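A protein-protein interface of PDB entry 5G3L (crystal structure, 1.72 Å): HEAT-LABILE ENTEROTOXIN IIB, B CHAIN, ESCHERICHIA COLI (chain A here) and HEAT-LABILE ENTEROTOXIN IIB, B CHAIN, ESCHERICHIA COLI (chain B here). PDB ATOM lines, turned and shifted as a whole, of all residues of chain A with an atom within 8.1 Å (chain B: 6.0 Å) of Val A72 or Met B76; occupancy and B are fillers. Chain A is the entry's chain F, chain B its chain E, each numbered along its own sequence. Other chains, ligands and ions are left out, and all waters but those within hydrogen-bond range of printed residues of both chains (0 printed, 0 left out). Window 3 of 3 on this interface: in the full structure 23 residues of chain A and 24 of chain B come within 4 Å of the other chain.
OE1 of Glu B97 is in salt-bridge range of NZ of Lys A25, 3.0 Å away. The backbone NH of Leu B96 sits at hydrogen-bond distance from the backbone carbonyl oxygen of Tyr A26 (2.8 Å). The backbone carbonyl oxygen of Thr A24 sits at hydrogen-bond distance from the backbone NH of Ala B98, 2.8 Å away.
O of Lys A25 sits at hydrogen-bond distance from N of Val A40 (3.0 Å). The backbone NH (N) of Glu B97 sits at hydrogen-bond distance from the backbone carbonyl oxygen (O) of Arg B77 (3.1 Å). The backbone NH of Met B76 lies within hydrogen-bond range of the side-chain hydroxyl of Ser B74 (3.0 Å). The backbone NH of Thr A24 lies within hydrogen-bond range of the backbone carbonyl oxygen of Val A40 (2.9 Å).
O of Thr A24 touches O of Leu B96, 3.8 Å away. Glu B97 touches Thr A24 (CA to O, 3.4 Å). Leu B96 touches Lys A25. Met A69 touches Leu B96. O of Val A72 touches CE of Met B76, at 3.6 Å. Ala B98 touches Val A72. SD of Met B76 touches CD2 of Leu A73 (3.5 Å).
Of the printed residues of chain B, Tyr A26 touches Leu B96. Val A72 touches just these residues of chain B: Met B76 and Ala B98. Of the printed residues of chain B, Leu A73 touches Met B76. Val B21 touches none of the printed residues of chain A. No residue of chain A comes within 4 Å of Gly B75. Met B76 touches just these residues of chain A: Val A72 (3.6 Å) and Leu A73 (3.5 Å). Printed residues of chain A within 4 Å of Leu B96: Thr A24, Lys A25, Tyr A26 and Met A69. The nearest residue of chain B that does not touch Val A72 is Leu B96 (4.2 Å). The nearest residue of chain A that does not touch Met B76 is Ser A74 (5.4 Å).
Hydrophobic or aromatic side chains of chain B within 4 Å of the printed part of chain A: Met B76, Leu B96 and Ala B98. Of the 25 printed residues of chain A, 6 touch a printed residue of chain B. Among the printed residues, 10 pairs touch across the chains. Among the printed residues, Asp or Glu carboxylates within 4 Å of a Lys or Arg side-chain nitrogen of the other chain: Lys A25 with Glu B97.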
ATOM      1  N   GLU A  22      -0.888 -27.346 -22.362  1.00  0.00           N
ATOM      2  CA  GLU A  22       0.352 -26.739 -21.885  1.00  0.00           C
ATOM      3  C   GLU A  22      -0.007 -25.554 -21.005  1.00  0.00           C
ATOM      4  O   GLU A  22      -0.544 -24.558 -21.465  1.00  0.00           O
ATOM      5  CB  GLU A  22       1.238 -26.243 -23.032  1.00  0.00           C
ATOM      6  CG  GLU A  22       2.635 -25.795 -22.560  1.00  0.00           C
ATOM      7  CD  GLU A  22       3.489 -25.145 -23.659  1.00  0.00           C
ATOM      8  OE1 GLU A  22       2.938 -24.644 -24.671  1.00  0.00           O
ATOM      9  OE2 GLU A  22       4.710 -25.084 -23.466  1.00  0.00           O
ATOM     10  N   LEU A  23       0.312 -25.657 -19.729  1.00  0.00           N
ATOM     11  CA  LEU A  23       0.054 -24.554 -18.783  1.00  0.00           C
ATOM     12  C   LEU A  23       1.286 -23.667 -18.757  1.00  0.00           C
ATOM     13  O   LEU A  23       2.395 -24.137 -18.511  1.00  0.00           O
ATOM     14  CB  LEU A  23      -0.245 -25.067 -17.367  1.00  0.00           C
ATOM     15  CG  LEU A  23      -1.469 -25.985 -17.263  1.00  0.00           C
ATOM     16  CD1 LEU A  23      -1.654 -26.437 -15.814  1.00  0.00           C
ATOM     17  CD2 LEU A  23      -2.725 -25.336 -17.759  1.00  0.00           C
ATOM     18  N   THR A  24       1.063 -22.391 -18.999  1.00  0.00           N
ATOM     19  CA  THR A  24       2.113 -21.411 -19.058  1.00  0.00           C
ATOM     20  C   THR A  24       2.068 -20.328 -17.956  1.00  0.00           C
ATOM     21  O   THR A  24       3.051 -19.588 -17.810  1.00  0.00           O
ATOM     22  CB  THR A  24       2.171 -20.709 -20.439  1.00  0.00           C
ATOM     23  OG1 THR A  24       0.929 -20.069 -20.709  1.00  0.00           O
ATOM     24  CG2 THR A  24       2.457 -21.766 -21.510  1.00  0.00           C
ATOM     25  N   LYS A  25       0.966 -20.227 -17.239  1.00  0.00           N
ATOM     26  CA  LYS A  25       0.819 -19.289 -16.125  1.00  0.00           C
ATOM     27  C   LYS A  25       0.141 -19.939 -14.929  1.00  0.00           C
ATOM     28  O   LYS A  25      -0.810 -20.687 -15.072  1.00  0.00           O
ATOM     29  CB  LYS A  25       0.100 -18.029 -16.539  1.00  0.00           C
ATOM     30  CG  LYS A  25       0.704 -17.407 -17.822  1.00  0.00           C
ATOM     31  CD  LYS A  25       0.277 -15.989 -18.050  1.00  0.00           C
ATOM     32  CE  LYS A  25       0.529 -15.496 -19.474  1.00  0.00           C
ATOM     33  NZ  LYS A  25       1.934 -15.157 -19.727  1.00  0.00           N
ATOM     34  N   TYR A  26       0.576 -19.537 -13.751  1.00  0.00           N
ATOM     35  CA  TYR A  26      -0.072 -19.931 -12.474  1.00  0.00           C
ATOM     36  C   TYR A  26      -0.310 -18.681 -11.598  1.00  0.00           C
ATOM     37  O   TYR A  26       0.601 -17.882 -11.392  1.00  0.00           O
ATOM     38  CB  TYR A  26       0.868 -20.870 -11.769  1.00  0.00           C
ATOM     39  CG  TYR A  26       0.416 -21.459 -10.453  1.00  0.00           C
ATOM     40  CD1 TYR A  26      -0.778 -22.099 -10.327  1.00  0.00           C
ATOM     41  CD2 TYR A  26       1.248 -21.403  -9.330  1.00  0.00           C
ATOM     42  CE1 TYR A  26      -1.126 -22.716  -9.144  1.00  0.00           C
ATOM     43  CE2 TYR A  26       0.900 -22.012  -8.159  1.00  0.00           C
ATOM     44  CZ  TYR A  26      -0.284 -22.688  -8.094  1.00  0.00           C
ATOM     45  OH  TYR A  26      -0.676 -23.341  -6.922  1.00  0.00           O
ATOM     46  N   ILE A  27      -1.538 -18.548 -11.105  1.00  0.00           N
ATOM     47  CA  ILE A  27      -2.038 -17.370 -10.397  1.00  0.00           C
ATOM     48  C   ILE A  27      -2.513 -17.670  -8.975  1.00  0.00           C
ATOM     49  O   ILE A  27      -3.315 -18.571  -8.801  1.00  0.00           O
ATOM     50  CB  ILE A  27      -3.211 -16.695 -11.171  1.00  0.00           C
ATOM     51  CG1 ILE A  27      -2.825 -16.264 -12.597  1.00  0.00           C
ATOM     52  CG2 ILE A  27      -3.734 -15.507 -10.348  1.00  0.00           C
ATOM     53  CD1 ILE A  27      -4.000 -15.893 -13.491  1.00  0.00           C
ATOM     54  N   TYR A  38      -5.557 -20.176  -9.965  1.00  0.00           N
ATOM     55  CA  TYR A  38      -5.904 -20.352 -11.386  1.00  0.00           C
ATOM     56  C   TYR A  38      -4.696 -20.746 -12.241  1.00  0.00           C
ATOM     57  O   TYR A  38      -3.526 -20.459 -11.909  1.00  0.00           O
ATOM     58  CB  TYR A  38      -6.525 -19.101 -11.989  1.00  0.00           C
ATOM     59  CG  TYR A  38      -7.657 -18.552 -11.178  1.00  0.00           C
ATOM     60  CD1 TYR A  38      -7.397 -17.634 -10.177  1.00  0.00           C
ATOM     61  CD2 TYR A  38      -8.984 -18.845 -11.478  1.00  0.00           C
ATOM     62  CE1 TYR A  38      -8.428 -17.065  -9.454  1.00  0.00           C
ATOM     63  CE2 TYR A  38     -10.012 -18.286 -10.746  1.00  0.00           C
ATOM     64  CZ  TYR A  38      -9.730 -17.403  -9.724  1.00  0.00           C
ATOM     65  OH  TYR A  38     -10.748 -16.764  -8.988  1.00  0.00           O
ATOM     66  N   VAL A  39      -4.982 -21.462 -13.314  1.00  0.00           N
ATOM     67  CA  VAL A  39      -3.961 -21.729 -14.334  1.00  0.00           C
ATOM     68  C   VAL A  39      -4.437 -21.201 -15.714  1.00  0.00           C
ATOM     69  O   VAL A  39      -5.622 -21.107 -15.979  1.00  0.00           O
ATOM     70  CB  VAL A  39      -3.638 -23.213 -14.460  1.00  0.00           C
ATOM     71  CG1 VAL A  39      -3.004 -23.766 -13.180  1.00  0.00           C
ATOM     72  CG2 VAL A  39      -4.873 -24.040 -14.817  1.00  0.00           C
ATOM     73  N   VAL A  40      -3.458 -20.829 -16.536  1.00  0.00           N
ATOM     74  CA  VAL A  40      -3.691 -20.303 -17.882  1.00  0.00           C
ATOM     75  C   VAL A  40      -2.882 -21.151 -18.846  1.00  0.00           C
ATOM     76  O   VAL A  40      -1.683 -21.410 -18.627  1.00  0.00           O
ATOM     77  CB  VAL A  40      -3.265 -18.820 -18.026  1.00  0.00           C
ATOM     78  CG1 VAL A  40      -3.736 -18.294 -19.363  1.00  0.00           C
ATOM     79  CG2 VAL A  40      -3.839 -17.963 -16.876  1.00  0.00           C
ATOM     80  N   SER A  41      -3.523 -21.550 -19.951  1.00  0.00           N
ATOM     81  CA  SER A  41      -2.825 -22.334 -20.928  1.00  0.00           C
ATOM     82  C   SER A  41      -2.083 -21.471 -21.991  1.00  0.00           C
ATOM     83  O   SER A  41      -2.317 -20.276 -22.103  1.00  0.00           O
ATOM     84  CB  SER A  41      -3.782 -23.295 -21.667  1.00  0.00           C
ATOM     85  OG  SER A  41      -4.652 -22.577 -22.561  1.00  0.00           O
ATOM     86  N   ARG A  65      -2.635 -28.220  -6.942  1.00  0.00           N
ATOM     87  CA  ARG A  65      -1.743 -27.018  -6.963  1.00  0.00           C
ATOM     88  C   ARG A  65      -0.304 -27.396  -7.237  1.00  0.00           C
ATOM     89  O   ARG A  65       0.392 -26.731  -7.979  1.00  0.00           O
ATOM     90  CB  ARG A  65      -1.853 -26.250  -5.637  1.00  0.00           C
ATOM     91  CG  ARG A  65      -3.215 -25.664  -5.406  1.00  0.00           C
ATOM     92  CD  ARG A  65      -3.209 -24.690  -4.193  1.00  0.00           C
ATOM     93  NE  ARG A  65      -2.824 -25.295  -2.950  1.00  0.00           N
ATOM     94  CZ  ARG A  65      -3.690 -25.845  -2.090  1.00  0.00           C
ATOM     95  NH1 ARG A  65      -4.976 -25.908  -2.399  1.00  0.00           N
ATOM     96  NH2 ARG A  65      -3.268 -26.350  -0.976  1.00  0.00           N
ATOM     97  N   LYS A  66       0.157 -28.522  -6.671  1.00  0.00           N
ATOM     98  CA  LYS A  66       1.504 -29.014  -6.955  1.00  0.00           C
ATOM     99  C   LYS A  66       1.671 -29.427  -8.417  1.00  0.00           C
ATOM    100  O   LYS A  66       2.715 -29.139  -9.021  1.00  0.00           O
ATOM    101  CB  LYS A  66       1.900 -30.149  -6.035  1.00  0.00           C
ATOM    102  CG  LYS A  66       2.004 -29.748  -4.566  1.00  0.00           C
ATOM    103  CD  LYS A  66       2.282 -30.942  -3.651  1.00  0.00           C
ATOM    104  CE  LYS A  66       2.045 -30.578  -2.200  1.00  0.00           C
ATOM    105  NZ  LYS A  66       2.157 -31.791  -1.347  1.00  0.00           N
ATOM    106  N   ILE A  67       0.649 -30.073  -8.956  1.00  0.00           N
ATOM    107  CA  ILE A  67       0.662 -30.483 -10.381  1.00  0.00           C
ATOM    108  C   ILE A  67       0.766 -29.217 -11.257  1.00  0.00           C
ATOM    109  O   ILE A  67       1.516 -29.154 -12.217  1.00  0.00           O
ATOM    110  CB  ILE A  67      -0.567 -31.375 -10.667  1.00  0.00           C
ATOM    111  CG1 ILE A  67      -0.347 -32.808 -10.115  1.00  0.00           C
ATOM    112  CG2 ILE A  67      -0.866 -31.405 -12.135  1.00  0.00           C
ATOM    113  CD1 ILE A  67      -1.610 -33.658 -10.081  1.00  0.00           C
ATOM    114  N   ALA A  68      -0.063 -28.235 -10.943  1.00  0.00           N
ATOM    115  CA  ALA A  68      -0.075 -26.964 -11.721  1.00  0.00           C
ATOM    116  C   ALA A  68       1.284 -26.306 -11.742  1.00  0.00           C
ATOM    117  O   ALA A  68       1.769 -25.939 -12.808  1.00  0.00           O
ATOM    118  CB  ALA A  68      -1.099 -26.029 -11.118  1.00  0.00           C
ATOM    119  N   MET A  69       1.901 -26.153 -10.589  1.00  0.00           N
ATOM    120  CA  MET A  69       3.205 -25.521 -10.549  1.00  0.00           C
ATOM    121  C   MET A  69       4.223 -26.358 -11.309  1.00  0.00           C
ATOM    122  O   MET A  69       5.056 -25.810 -12.013  1.00  0.00           O
ATOM    123  CB  MET A  69       3.693 -25.355  -9.121  1.00  0.00           C
ATOM    124  CG  MET A  69       5.134 -24.860  -9.016  1.00  0.00           C
ATOM    125  SD  MET A  69       5.223 -23.063  -8.986  1.00  0.00           S
ATOM    126  CE  MET A  69       4.474 -22.938  -7.334  1.00  0.00           C
ATOM    127  N   ALA A  70       4.205 -27.666 -11.099  1.00  0.00           N
ATOM    128  CA  ALA A  70       5.172 -28.556 -11.779  1.00  0.00           C
ATOM    129  C   ALA A  70       5.037 -28.471 -13.290  1.00  0.00           C
ATOM    130  O   ALA A  70       6.050 -28.504 -14.009  1.00  0.00           O
ATOM    131  CB  ALA A  70       4.996 -29.978 -11.323  1.00  0.00           C
ATOM    132  N   ALA A  71       3.810 -28.374 -13.772  1.00  0.00           N
ATOM    133  CA  ALA A  71       3.531 -28.247 -15.214  1.00  0.00           C
ATOM    134  C   ALA A  71       4.059 -26.934 -15.759  1.00  0.00           C
ATOM    135  O   ALA A  71       4.652 -26.892 -16.847  1.00  0.00           O
ATOM    136  CB  ALA A  71       2.040 -28.368 -15.479  1.00  0.00           C
ATOM    137  N   VAL A  72       3.798 -25.831 -15.027  1.00  0.00           N
ATOM    138  CA  VAL A  72       4.306 -24.501 -15.454  1.00  0.00           C
ATOM    139  C   VAL A  72       5.834 -24.466 -15.495  1.00  0.00           C
ATOM    140  O   VAL A  72       6.429 -23.993 -16.487  1.00  0.00           O
ATOM    141  CB  VAL A  72       3.701 -23.366 -14.611  1.00  0.00           C
ATOM    142  CG1 VAL A  72       4.406 -22.027 -14.869  1.00  0.00           C
ATOM    143  CG2 VAL A  72       2.207 -23.254 -14.859  1.00  0.00           C
ATOM    144  N   LEU A  73       6.468 -25.010 -14.477  1.00  0.00           N
ATOM    145  CA  LEU A  73       7.947 -25.029 -14.414  1.00  0.00           C
ATOM    146  C   LEU A  73       8.613 -25.873 -15.477  1.00  0.00           C
ATOM    147  O   LEU A  73       9.618 -25.449 -16.047  1.00  0.00           O
ATOM    148  CB  LEU A  73       8.425 -25.455 -13.040  1.00  0.00           C
ATOM    149  CG  LEU A  73       8.170 -24.363 -11.959  1.00  0.00           C
ATOM    150  CD1 LEU A  73       8.672 -24.932 -10.643  1.00  0.00           C
ATOM    151  CD2 LEU A  73       8.771 -22.943 -12.194  1.00  0.00           C
ATOM    152  N   SER A  74       8.013 -27.011 -15.801  1.00  0.00           N
ATOM    153  CA  SER A  74       8.630 -28.053 -16.651  1.00  0.00           C
ATOM    154  C   SER A  74       8.159 -28.030 -18.102  1.00  0.00           C
ATOM    155  O   SER A  74       8.847 -28.562 -18.976  1.00  0.00           O
ATOM    156  CB  SER A  74       8.356 -29.427 -16.081  1.00  0.00           C
ATOM    157  OG  SER A  74       6.962 -29.784 -16.220  1.00  0.00           O
ATOM    158  N   GLY A  75       6.995 -27.448 -18.351  1.00  0.00           N
ATOM    159  CA  GLY A  75       6.330 -27.587 -19.670  1.00  0.00           C
ATOM    160  C   GLY A  75       5.675 -28.953 -19.922  1.00  0.00           C
ATOM    161  O   GLY A  75       5.162 -29.193 -21.004  1.00  0.00           O
ATOM    162  N   MET A  76       5.611 -29.819 -18.913  1.00  0.00           N
ATOM    163  CA  MET A  76       4.851 -31.062 -18.997  1.00  0.00           C
ATOM    164  C   MET A  76       3.372 -30.777 -19.183  1.00  0.00           C
ATOM    165  O   MET A  76       2.835 -29.872 -18.556  1.00  0.00           O
ATOM    166  CB  MET A  76       4.995 -31.904 -17.715  1.00  0.00           C
ATOM    167  CG  MET A  76       6.281 -32.662 -17.640  1.00  0.00           C
ATOM    168  SD  MET A  76       6.334 -33.729 -16.150  1.00  0.00           S
ATOM    169  CE  MET A  76       7.877 -34.570 -16.490  1.00  0.00           C
ATOM    170  N   ARG A  77       2.722 -31.554 -20.034  1.00  0.00           N
ATOM    171  CA  ARG A  77       1.326 -31.374 -20.324  1.00  0.00           C
ATOM    172  C   ARG A  77       0.444 -31.943 -19.218  1.00  0.00           C
ATOM    173  O   ARG A  77       0.866 -32.817 -18.456  1.00  0.00           O
ATOM    174  CB  ARG A  77       0.973 -32.037 -21.649  1.00  0.00           C
ATOM    175  CG  ARG A  77       1.925 -31.642 -22.772  1.00  0.00           C
ATOM    176  CD  ARG A  77       1.324 -30.697 -23.734  1.00  0.00           C
ATOM    177  NE  ARG A  77       2.321 -29.893 -24.464  1.00  0.00           N
ATOM    178  CZ  ARG A  77       2.032 -29.111 -25.504  1.00  0.00           C
ATOM    179  NH1 ARG A  77       0.788 -29.036 -25.985  1.00  0.00           N
ATOM    180  NH2 ARG A  77       2.994 -28.383 -26.063  1.00  0.00           N
ATOM    181  N   VAL A  78      -0.768 -31.431 -19.143  1.00  0.00           N
ATOM    182  CA  VAL A  78      -1.796 -31.979 -18.275  1.00  0.00           C
ATOM    183  C   VAL A  78      -3.073 -32.358 -19.089  1.00  0.00           C
ATOM    184  O   VAL A  78      -3.383 -31.778 -20.139  1.00  0.00           O
ATOM    185  CB  VAL A  78      -2.207 -31.014 -17.142  1.00  0.00           C
ATOM    186  CG1 VAL A  78      -0.972 -30.679 -16.298  1.00  0.00           C
ATOM    187  CG2 VAL A  78      -2.834 -29.759 -17.692  1.00  0.00           C
ATOM    188  N   LEU A  96      -1.184 -35.131 -14.555  1.00  0.00           N
ATOM    189  CA  LEU A  96       0.127 -34.660 -15.037  1.00  0.00           C
ATOM    190  C   LEU A  96       0.810 -35.753 -15.821  1.00  0.00           C
ATOM    191  O   LEU A  96       0.863 -36.898 -15.354  1.00  0.00           O
ATOM    192  CB  LEU A  96       1.039 -34.323 -13.858  1.00  0.00           C
ATOM    193  CG  LEU A  96       2.444 -33.795 -14.156  1.00  0.00           C
ATOM    194  CD1 LEU A  96       2.420 -32.462 -14.840  1.00  0.00           C
ATOM    195  CD2 LEU A  96       3.225 -33.696 -12.839  1.00  0.00           C
ATOM    196  N   VAL B  21       8.385  -8.865 -14.275  1.00  0.00           N
ATOM    197  CA  VAL B  21       9.388  -8.617 -13.230  1.00  0.00           C
ATOM    198  C   VAL B  21      10.282  -9.845 -13.066  1.00  0.00           C
ATOM    199  O   VAL B  21       9.780 -10.998 -12.944  1.00  0.00           O
ATOM    200  CB  VAL B  21       8.709  -8.237 -11.912  1.00  0.00           C
ATOM    201  CG1 VAL B  21       9.742  -7.932 -10.853  1.00  0.00           C
ATOM    202  CG2 VAL B  21       7.780  -7.040 -12.057  1.00  0.00           C
ATOM    203  N   GLU B  22      11.625  -9.654 -13.068  1.00  0.00           N
ATOM    204  CA  GLU B  22      12.581 -10.727 -12.758  1.00  0.00           C
ATOM    205  C   GLU B  22      12.932 -10.612 -11.271  1.00  0.00           C
ATOM    206  O   GLU B  22      13.512  -9.629 -10.868  1.00  0.00           O
ATOM    207  CB  GLU B  22      13.867 -10.640 -13.601  1.00  0.00           C
ATOM    208  CG  GLU B  22      14.783 -11.832 -13.384  1.00  0.00           C
ATOM    209  CD  GLU B  22      16.151 -11.729 -14.066  1.00  0.00           C
ATOM    210  OE1 GLU B  22      16.611 -10.605 -14.366  1.00  0.00           O
ATOM    211  OE2 GLU B  22      16.811 -12.760 -14.210  1.00  0.00           O
ATOM    212  N   LEU B  23      12.557 -11.605 -10.466  1.00  0.00           N
ATOM    213  CA  LEU B  23      12.838 -11.615  -9.036  1.00  0.00           C
ATOM    214  C   LEU B  23      14.182 -12.320  -8.840  1.00  0.00           C
ATOM    215  O   LEU B  23      14.364 -13.423  -9.312  1.00  0.00           O
ATOM    216  CB  LEU B  23      11.757 -12.325  -8.208  1.00  0.00           C
ATOM    217  CG  LEU B  23      10.347 -11.722  -8.364  1.00  0.00           C
ATOM    218  CD1 LEU B  23       9.391 -12.523  -7.503  1.00  0.00           C
ATOM    219  CD2 LEU B  23      10.327 -10.258  -7.944  1.00  0.00           C
ATOM    220  N   ALA B  70      10.087 -20.065  -6.619  1.00  0.00           N
ATOM    221  CA  ALA B  70      10.250 -20.684  -7.931  1.00  0.00           C
ATOM    222  C   ALA B  70      10.820 -19.701  -8.951  1.00  0.00           C
ATOM    223  O   ALA B  70      11.624 -20.078  -9.806  1.00  0.00           O
ATOM    224  CB  ALA B  70       8.950 -21.285  -8.406  1.00  0.00           C
ATOM    225  N   ALA B  71      10.348 -18.474  -8.861  1.00  0.00           N
ATOM    226  CA  ALA B  71      10.803 -17.373  -9.774  1.00  0.00           C
ATOM    227  C   ALA B  71      12.255 -17.035  -9.530  1.00  0.00           C
ATOM    228  O   ALA B  71      13.022 -16.876 -10.482  1.00  0.00           O
ATOM    229  CB  ALA B  71       9.943 -16.133  -9.580  1.00  0.00           C
ATOM    230  N   VAL B  72      12.636 -16.947  -8.257  1.00  0.00           N
ATOM    231  CA  VAL B  72      14.056 -16.653  -7.895  1.00  0.00           C
ATOM    232  C   VAL B  72      14.997 -17.776  -8.381  1.00  0.00           C
ATOM    233  O   VAL B  72      16.039 -17.535  -9.017  1.00  0.00           O
ATOM    234  CB  VAL B  72      14.217 -16.345  -6.396  1.00  0.00           C
ATOM    235  CG1 VAL B  72      15.689 -16.337  -5.998  1.00  0.00           C
ATOM    236  CG2 VAL B  72      13.554 -15.022  -6.026  1.00  0.00           C
ATOM    237  N   SER B  74      14.501 -19.982 -10.845  1.00  0.00           N
ATOM    238  CA  SER B  74      14.414 -20.288 -12.295  1.00  0.00           C
ATOM    239  C   SER B  74      14.705 -19.108 -13.224  1.00  0.00           C
ATOM    240  O   SER B  74      14.981 -19.310 -14.400  1.00  0.00           O
ATOM    241  CB  SER B  74      13.027 -20.868 -12.628  1.00  0.00           C
ATOM    242  OG  SER B  74      12.007 -19.854 -12.499  1.00  0.00           O
ATOM    243  N   GLY B  75      14.531 -17.911 -12.708  1.00  0.00           N
ATOM    244  CA  GLY B  75      14.527 -16.703 -13.519  1.00  0.00           C
ATOM    245  C   GLY B  75      13.233 -16.471 -14.309  1.00  0.00           C
ATOM    246  O   GLY B  75      13.172 -15.576 -15.125  1.00  0.00           O
ATOM    247  N   MET B  76      12.206 -17.260 -14.086  1.00  0.00           N
ATOM    248  CA  MET B  76      10.909 -17.035 -14.695  1.00  0.00           C
ATOM    249  C   MET B  76      10.358 -15.715 -14.182  1.00  0.00           C
ATOM    250  O   MET B  76      10.435 -15.426 -12.985  1.00  0.00           O
ATOM    251  CB  MET B  76       9.903 -18.128 -14.318  1.00  0.00           C
ATOM    252  CG  MET B  76      10.072 -19.390 -15.142  1.00  0.00           C
ATOM    253  SD  MET B  76       8.771 -20.605 -14.786  1.00  0.00           S
ATOM    254  CE  MET B  76       9.210 -21.793 -16.087  1.00  0.00           C
ATOM    255  N   ARG B  77       9.712 -14.990 -15.052  1.00  0.00           N
ATOM    256  CA  ARG B  77       9.115 -13.726 -14.695  1.00  0.00           C
ATOM    257  C   ARG B  77       7.793 -13.853 -13.998  1.00  0.00           C
ATOM    258  O   ARG B  77       7.134 -14.878 -14.102  1.00  0.00           O
ATOM    259  CB  ARG B  77       8.882 -12.863 -15.956  1.00  0.00           C
ATOM    260  CG  ARG B  77      10.073 -12.721 -16.836  1.00  0.00           C
ATOM    261  CD  ARG B  77      11.184 -12.119 -16.087  1.00  0.00           C
ATOM    262  NE  ARG B  77      12.154 -11.481 -16.972  1.00  0.00           N
ATOM    263  CZ  ARG B  77      13.358 -11.975 -17.277  1.00  0.00           C
ATOM    264  NH1 ARG B  77      13.778 -13.164 -16.805  1.00  0.00           N
ATOM    265  NH2 ARG B  77      14.154 -11.263 -18.061  1.00  0.00           N
ATOM    266  N   VAL B  78       7.445 -12.791 -13.242  1.00  0.00           N
ATOM    267  CA  VAL B  78       6.141 -12.676 -12.608  1.00  0.00           C
ATOM    268  C   VAL B  78       5.431 -11.370 -13.002  1.00  0.00           C
ATOM    269  O   VAL B  78       6.075 -10.339 -13.323  1.00  0.00           O
ATOM    270  CB  VAL B  78       6.193 -12.766 -11.074  1.00  0.00           C
ATOM    271  CG1 VAL B  78       6.845 -14.082 -10.637  1.00  0.00           C
ATOM    272  CG2 VAL B  78       6.989 -11.593 -10.488  1.00  0.00           C
ATOM    273  N   LEU B  96       2.873 -16.316 -12.047  1.00  0.00           N
ATOM    274  CA  LEU B  96       4.129 -16.869 -12.528  1.00  0.00           C
ATOM    275  C   LEU B  96       3.982 -17.247 -14.009  1.00  0.00           C
ATOM    276  O   LEU B  96       2.987 -17.901 -14.357  1.00  0.00           O
ATOM    277  CB  LEU B  96       4.453 -18.145 -11.727  1.00  0.00           C
ATOM    278  CG  LEU B  96       5.716 -18.905 -12.100  1.00  0.00           C
ATOM    279  CD1 LEU B  96       6.958 -18.080 -11.759  1.00  0.00           C
ATOM    280  CD2 LEU B  96       5.795 -20.214 -11.314  1.00  0.00           C
ATOM    281  N   GLU B  97       4.943 -16.878 -14.838  1.00  0.00           N
ATOM    282  CA  GLU B  97       4.849 -17.176 -16.249  1.00  0.00           C
ATOM    283  C   GLU B  97       6.047 -17.925 -16.827  1.00  0.00           C
ATOM    284  O   GLU B  97       7.197 -17.630 -16.542  1.00  0.00           O
ATOM    285  CB  GLU B  97       4.421 -15.958 -17.106  1.00  0.00           C
ATOM    286  CG  GLU B  97       5.336 -14.829 -17.097  1.00  0.00           C
ATOM    287  CD  GLU B  97       4.934 -13.733 -18.088  1.00  0.00           C
ATOM    288  OE1 GLU B  97       3.757 -13.328 -18.217  1.00  0.00           O
ATOM    289  OE2 GLU B  97       5.857 -13.207 -18.672  1.00  0.00           O
ATOM    290  N   ALA B  98       5.751 -18.972 -17.528  1.00  0.00           N
ATOM    291  CA  ALA B  98       6.768 -19.733 -18.228  1.00  0.00           C
ATOM    292  C   ALA B  98       7.291 -18.877 -19.433  1.00  0.00           C
ATOM    293  O   ALA B  98       8.422 -18.987 -19.836  1.00  0.00           O
ATOM    294  CB  ALA B  98       6.201 -21.082 -18.668  1.00  0.00           C
